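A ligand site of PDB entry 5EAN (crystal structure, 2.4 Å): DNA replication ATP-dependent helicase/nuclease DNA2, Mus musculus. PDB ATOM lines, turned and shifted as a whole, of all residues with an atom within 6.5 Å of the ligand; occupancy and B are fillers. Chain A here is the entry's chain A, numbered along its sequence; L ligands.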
ATOM      1  N   ARG A 139       0.555  -8.154 -36.825  1.00  0.00           N
ATOM      2  CA  ARG A 139       0.084  -7.214 -35.812  1.00  0.00           C
ATOM      3  C   ARG A 139       0.362  -7.692 -34.385  1.00  0.00           C
ATOM      4  O   ARG A 139       0.605  -6.874 -33.500  1.00  0.00           O
ATOM      5  CB  ARG A 139      -1.405  -6.869 -36.010  1.00  0.00           C
ATOM      6  CG  ARG A 139      -1.635  -5.644 -36.890  1.00  0.00           C
ATOM      7  CD  ARG A 139      -3.110  -5.318 -37.094  1.00  0.00           C
ATOM      8  NE  ARG A 139      -3.286  -4.331 -38.167  1.00  0.00           N
ATOM      9  CZ  ARG A 139      -3.707  -3.069 -38.015  1.00  0.00           C
ATOM     10  NH1 ARG A 139      -4.040  -2.587 -36.825  1.00  0.00           N
ATOM     11  NH2 ARG A 139      -3.823  -2.277 -39.083  1.00  0.00           N
ATOM     12  N   CYS A 140       0.333  -9.005 -34.150  1.00  0.00           N
ATOM     13  CA  CYS A 140       0.660  -9.518 -32.832  1.00  0.00           C
ATOM     14  C   CYS A 140       1.105 -10.985 -32.826  1.00  0.00           C
ATOM     15  O   CYS A 140       0.297 -11.925 -33.055  1.00  0.00           O
ATOM     16  CB  CYS A 140      -0.491  -9.328 -31.847  1.00  0.00           C
ATOM     17  SG  CYS A 140      -0.084 -10.068 -30.248  1.00  0.00           S
ATOM     18  N   LEU A 141       2.391 -11.179 -32.525  1.00  0.00           N
ATOM     19  CA  LEU A 141       2.983 -12.510 -32.423  1.00  0.00           C
ATOM     20  C   LEU A 141       2.323 -13.392 -31.361  1.00  0.00           C
ATOM     21  O   LEU A 141       2.159 -14.588 -31.533  1.00  0.00           O
ATOM     22  CB  LEU A 141       4.483 -12.412 -32.157  1.00  0.00           C
ATOM     23  CG  LEU A 141       5.297 -13.695 -32.380  1.00  0.00           C
ATOM     24  CD1 LEU A 141       5.179 -14.265 -33.789  1.00  0.00           C
ATOM     25  CD2 LEU A 141       6.753 -13.442 -32.024  1.00  0.00           C
ATOM     26  N   ARG A 142       1.938 -12.767 -30.262  1.00  0.00           N
ATOM     27  CA  ARG A 142       1.351 -13.457 -29.146  1.00  0.00           C
ATOM     28  C   ARG A 142      -0.057 -13.990 -29.503  1.00  0.00           C
ATOM     29  O   ARG A 142      -0.389 -15.132 -29.153  1.00  0.00           O
ATOM     30  CB  ARG A 142       1.338 -12.532 -27.942  1.00  0.00           C
ATOM     31  CG  ARG A 142       0.669 -13.088 -26.706  1.00  0.00           C
ATOM     32  CD  ARG A 142       0.529 -11.983 -25.698  1.00  0.00           C
ATOM     33  NE  ARG A 142      -0.004 -12.507 -24.435  1.00  0.00           N
ATOM     34  CZ  ARG A 142       0.742 -12.939 -23.420  1.00  0.00           C
ATOM     35  NH1 ARG A 142       2.073 -12.927 -23.500  1.00  0.00           N
ATOM     36  NH2 ARG A 142       0.153 -13.372 -22.316  1.00  0.00           N
ATOM     37  N   ARG A 143      -0.841 -13.172 -30.206  1.00  0.00           N
ATOM     38  CA  ARG A 143      -2.155 -13.544 -30.730  1.00  0.00           C
ATOM     39  C   ARG A 143      -2.066 -14.760 -31.626  1.00  0.00           C
ATOM     40  O   ARG A 143      -2.806 -15.722 -31.432  1.00  0.00           O
ATOM     41  CB  ARG A 143      -2.779 -12.381 -31.498  1.00  0.00           C
ATOM     42  CG  ARG A 143      -4.202 -12.662 -31.988  1.00  0.00           C
ATOM     43  CD  ARG A 143      -4.357 -12.269 -33.452  1.00  0.00           C
ATOM     44  NE  ARG A 143      -4.691 -10.866 -33.627  1.00  0.00           N
ATOM     45  CZ  ARG A 143      -4.175 -10.046 -34.553  1.00  0.00           C
ATOM     46  NH1 ARG A 143      -3.241 -10.474 -35.393  1.00  0.00           N
ATOM     47  NH2 ARG A 143      -4.563  -8.786 -34.622  1.00  0.00           N
ATOM     48  N   ALA A 144      -1.127 -14.740 -32.568  1.00  0.00           N
ATOM     49  CA  ALA A 144      -0.905 -15.894 -33.456  1.00  0.00           C
ATOM     50  C   ALA A 144      -0.618 -17.199 -32.704  1.00  0.00           C
ATOM     51  O   ALA A 144      -1.169 -18.236 -33.044  1.00  0.00           O
ATOM     52  CB  ALA A 144       0.179 -15.604 -34.464  1.00  0.00           C
ATOM     53  N   LEU A 146      -1.380 -17.891 -29.485  1.00  0.00           N
ATOM     54  CA  LEU A 146      -2.606 -18.224 -28.774  1.00  0.00           C
ATOM     55  C   LEU A 146      -3.672 -18.832 -29.690  1.00  0.00           C
ATOM     56  O   LEU A 146      -4.368 -19.752 -29.278  1.00  0.00           O
ATOM     57  CB  LEU A 146      -3.164 -17.016 -28.002  1.00  0.00           C
ATOM     58  CG  LEU A 146      -2.430 -16.630 -26.683  1.00  0.00           C
ATOM     59  CD1 LEU A 146      -2.848 -15.272 -26.133  1.00  0.00           C
ATOM     60  CD2 LEU A 146      -2.598 -17.699 -25.612  1.00  0.00           C
ATOM     61  N   GLN A 389       5.649 -11.059 -25.762  1.00  0.00           N
ATOM     62  CA  GLN A 389       5.131  -9.973 -24.943  1.00  0.00           C
ATOM     63  C   GLN A 389       3.757  -9.463 -25.405  1.00  0.00           C
ATOM     64  O   GLN A 389       3.466  -9.407 -26.595  1.00  0.00           O
ATOM     65  CB  GLN A 389       6.104  -8.791 -24.932  1.00  0.00           C
ATOM     66  CG  GLN A 389       7.514  -9.122 -24.496  1.00  0.00           C
ATOM     67  CD  GLN A 389       8.371  -7.873 -24.272  1.00  0.00           C
ATOM     68  OE1 GLN A 389       9.045  -7.753 -23.234  1.00  0.00           O
ATOM     69  NE2 GLN A 389       8.359  -6.931 -25.240  1.00  0.00           N
ATOM     70  N   ILE A 390       2.910  -9.113 -24.440  1.00  0.00           N
ATOM     71  CA  ILE A 390       1.757  -8.249 -24.677  1.00  0.00           C
ATOM     72  C   ILE A 390       2.232  -6.942 -25.380  1.00  0.00           C
ATOM     73  O   ILE A 390       3.228  -6.314 -24.963  1.00  0.00           O
ATOM     74  CB  ILE A 390       0.990  -7.989 -23.362  1.00  0.00           C
ATOM     75  CG1 ILE A 390       0.201  -9.250 -22.954  1.00  0.00           C
ATOM     76  CG2 ILE A 390       0.074  -6.783 -23.488  1.00  0.00           C
ATOM     77  CD1 ILE A 390      -0.145  -9.384 -21.478  1.00  0.00           C
ATOM     78  N   ILE A 391       1.528  -6.567 -26.451  1.00  0.00           N
ATOM     79  CA  ILE A 391       1.918  -5.438 -27.320  1.00  0.00           C
ATOM     80  C   ILE A 391       1.412  -4.091 -26.796  1.00  0.00           C
ATOM     81  O   ILE A 391       0.549  -4.029 -25.918  1.00  0.00           O
ATOM     82  CB  ILE A 391       1.482  -5.639 -28.805  1.00  0.00           C
ATOM     83  CG1 ILE A 391      -0.023  -5.948 -28.916  1.00  0.00           C
ATOM     84  CG2 ILE A 391       2.349  -6.700 -29.480  1.00  0.00           C
ATOM     85  CD1 ILE A 391      -0.648  -5.474 -30.196  1.00  0.00           C
ATOM     86  N   GLU A 393      -0.046  -1.659 -28.798  1.00  0.00           N
ATOM     87  CA  GLU A 393      -1.184  -1.164 -29.604  1.00  0.00           C
ATOM     88  C   GLU A 393      -2.572  -1.470 -29.023  1.00  0.00           C
ATOM     89  O   GLU A 393      -3.055  -2.608 -29.076  1.00  0.00           O
ATOM     90  CB  GLU A 393      -1.087  -1.655 -31.061  1.00  0.00           C
ATOM     91  CG  GLU A 393       0.312  -1.972 -31.587  1.00  0.00           C
ATOM     92  CD  GLU A 393       1.224  -0.758 -31.678  1.00  0.00           C
ATOM     93  OE1 GLU A 393       1.439  -0.263 -32.811  1.00  0.00           O
ATOM     94  OE2 GLU A 393       1.725  -0.284 -30.634  1.00  0.00           O
ATOM     95  N   THR A 396      -5.318  -2.796 -31.600  1.00  0.00           N
ATOM     96  CA  THR A 396      -5.157  -4.235 -31.891  1.00  0.00           C
ATOM     97  C   THR A 396      -5.811  -5.115 -30.805  1.00  0.00           C
ATOM     98  O   THR A 396      -6.625  -5.988 -31.130  1.00  0.00           O
ATOM     99  CB  THR A 396      -3.654  -4.638 -32.089  1.00  0.00           C
ATOM    100  OG1 THR A 396      -2.950  -3.628 -32.819  1.00  0.00           O
ATOM    101  CG2 THR A 396      -3.520  -5.956 -32.853  1.00  0.00           C
ATOM    102  N   CYS A 397      -5.476  -4.847 -29.545  1.00  0.00           N
ATOM    103  CA  CYS A 397      -5.962  -5.619 -28.391  1.00  0.00           C
ATOM    104  C   CYS A 397      -7.478  -5.579 -28.199  1.00  0.00           C
ATOM    105  O   CYS A 397      -8.104  -6.594 -27.892  1.00  0.00           O
ATOM    106  CB  CYS A 397      -5.276  -5.146 -27.110  1.00  0.00           C
ATOM    107  SG  CYS A 397      -3.486  -5.355 -27.122  1.00  0.00           S
ATOM    108  N   LYS A 398      -8.049  -4.389 -28.395  1.00  0.00           N
ATOM    109  CA  LYS A 398      -9.500  -4.144 -28.292  1.00  0.00           C
ATOM    110  C   LYS A 398     -10.310  -5.082 -29.216  1.00  0.00           C
ATOM    111  O   LYS A 398     -11.329  -5.631 -28.801  1.00  0.00           O
ATOM    112  CB  LYS A 398      -9.778  -2.666 -28.590  1.00  0.00           C
ATOM    113  CG  LYS A 398     -11.226  -2.233 -28.440  1.00  0.00           C
ATOM    114  CD  LYS A 398     -11.526  -1.142 -29.453  1.00  0.00           C
ATOM    115  CE  LYS A 398     -12.998  -1.120 -29.814  1.00  0.00           C
ATOM    116  NZ  LYS A 398     -13.240  -0.024 -30.802  1.00  0.00           N
ATOM    117  N   CYS A 400      -9.156  -7.938 -30.445  1.00  0.00           N
ATOM    118  CA  CYS A 400      -8.578  -9.280 -30.357  1.00  0.00           C
ATOM    119  C   CYS A 400      -9.462 -10.322 -29.644  1.00  0.00           C
ATOM    120  O   CYS A 400      -9.837 -10.145 -28.474  1.00  0.00           O
ATOM    121  CB  CYS A 400      -7.186  -9.265 -29.717  1.00  0.00           C
ATOM    122  SG  CYS A 400      -6.428 -10.909 -29.581  1.00  0.00           S
ATOM    123  N   SER A 401      -9.735 -11.399 -30.363  1.00  0.00           N
ATOM    124  CA  SER A 401     -10.590 -12.506 -29.895  1.00  0.00           C
ATOM    125  C   SER A 401      -9.881 -13.430 -28.887  1.00  0.00           C
ATOM    126  O   SER A 401     -10.529 -14.252 -28.213  1.00  0.00           O
ATOM    127  CB  SER A 401     -11.055 -13.326 -31.100  1.00  0.00           C
ATOM    128  OG  SER A 401      -9.925 -13.710 -31.872  1.00  0.00           O
ATOM    129  N   GLN A 402      -8.554 -13.309 -28.799  1.00  0.00           N
ATOM    130  CA  GLN A 402      -7.772 -14.082 -27.839  1.00  0.00           C
ATOM    131  C   GLN A 402      -7.520 -13.368 -26.500  1.00  0.00           C
ATOM    132  O   GLN A 402      -6.773 -13.878 -25.672  1.00  0.00           O
ATOM    133  CB  GLN A 402      -6.455 -14.526 -28.501  1.00  0.00           C
ATOM    134  CG  GLN A 402      -6.580 -15.650 -29.526  1.00  0.00           C
ATOM    135  CD  GLN A 402      -6.980 -17.005 -28.926  1.00  0.00           C
ATOM    136  OE1 GLN A 402      -6.763 -17.281 -27.741  1.00  0.00           O
ATOM    137  NE2 GLN A 402      -7.575 -17.866 -29.773  1.00  0.00           N
ATOM    138  N   ILE A 403      -8.158 -12.230 -26.262  1.00  0.00           N
ATOM    139  CA  ILE A 403      -7.904 -11.437 -25.030  1.00  0.00           C
ATOM    140  C   ILE A 403      -8.119 -12.222 -23.728  1.00  0.00           C
ATOM    141  O   ILE A 403      -7.368 -12.031 -22.763  1.00  0.00           O
ATOM    142  CB  ILE A 403      -8.656 -10.056 -25.021  1.00  0.00           C
ATOM    143  CG1 ILE A 403      -8.186  -9.171 -23.843  1.00  0.00           C
ATOM    144  CG2 ILE A 403     -10.177 -10.229 -25.030  1.00  0.00           C
ATOM    145  CD1 ILE A 403      -8.251  -7.666 -24.094  1.00  0.00           C
ATOM    146  N   CYS A 406      -5.222 -14.469 -23.381  1.00  0.00           N
ATOM    147  CA  CYS A 406      -4.069 -13.596 -23.213  1.00  0.00           C
ATOM    148  C   CYS A 406      -3.949 -13.151 -21.753  1.00  0.00           C
ATOM    149  O   CYS A 406      -2.909 -13.340 -21.134  1.00  0.00           O
ATOM    150  CB  CYS A 406      -4.152 -12.402 -24.160  1.00  0.00           C
ATOM    151  SG  CYS A 406      -2.834 -11.171 -23.951  1.00  0.00           S
ATOM    152  N   ALA A 407      -5.030 -12.593 -21.219  1.00  0.00           N
ATOM    153  CA  ALA A 407      -5.073 -12.147 -19.841  1.00  0.00           C
ATOM    154  C   ALA A 407      -4.852 -13.321 -18.875  1.00  0.00           C
ATOM    155  O   ALA A 407      -4.082 -13.227 -17.939  1.00  0.00           O
ATOM    156  CB  ALA A 407      -6.394 -11.456 -19.562  1.00  0.00           C
ATOM    157  N   MET A 426      -3.728  -1.986 -20.491  1.00  0.00           N
ATOM    158  CA  MET A 426      -3.785  -3.417 -20.731  1.00  0.00           C
ATOM    159  C   MET A 426      -3.644  -4.171 -19.400  1.00  0.00           C
ATOM    160  O   MET A 426      -4.227  -5.248 -19.214  1.00  0.00           O
ATOM    161  CB  MET A 426      -2.703  -3.811 -21.740  1.00  0.00           C
ATOM    162  CG  MET A 426      -2.814  -5.218 -22.280  1.00  0.00           C
ATOM    163  SD  MET A 426      -4.338  -5.643 -23.135  1.00  0.00           S
ATOM    164  CE  MET A 426      -4.118  -7.402 -23.393  1.00  0.00           C
HETATM  165 FE1  LIG L   1      -1.707  -9.716 -28.663  1.00  0.00          FE
HETATM  166 FE2  LIG L   1      -2.991 -10.187 -26.026  1.00  0.00          FE
HETATM  167 FE3  LIG L   1      -4.554 -10.150 -28.489  1.00  0.00          FE
HETATM  168 FE4  LIG L   1      -3.313  -7.640 -27.454  1.00  0.00          FE
HETATM  169  S1  LIG L   1      -4.706  -9.080 -26.646  1.00  0.00           S
HETATM  170  S2  LIG L   1      -3.375  -8.593 -29.386  1.00  0.00           S
HETATM  171  S3  LIG L   1      -1.601  -8.719 -26.765  1.00  0.00           S
HETATM  172  S4  LIG L   1      -2.891 -11.305 -27.846  1.00  0.00           S
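Arg 142 touches the ligand (CD to FE2, 3.97 Å). Ile 390 touches the ligand (CA to S3, 3.98 Å). N of Ile 391 touches S3 of the ligand (3.8 Å). CE of Met 426 touches S1 of the ligand (3.7 Å). Hydrophobic or aromatic side chains that line the ligand: Ile 391 and Met 426. Of the 21 residues printed, 9 come within 4 Å of the ligand. The nearest printed residue that does not touch the ligand is Ile 403 (4.3 Å).
SG of Cys 140 binds FE1 of the ligand (2.3 Å). SG of Cys 406 is bound to FE2 of the ligand. FE3 of the ligand is bound by SG of Cys 400. SG of Cys 397 binds FE4 of the ligand (2.3 Å). S4 of the ligand lies close to N of Arg 143 (3.6 Å).
N of Gln 402 lies close to SG of Cys 400 (3.3 Å). O of Cys 406 sits at hydrogen-bond distance from NH2 of Arg 142. O of Glu 393 lies close to SG of Cys 397 (3.4 Å). The side-chain sulfur (SG) of Cys 140 sits close to the backbone NH (N) of Arg 143 (3.2 Å). The side-chain sulfur (SG) of Cys 140 sits close to the backbone NH (N) of Arg 142 (3.4 Å).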
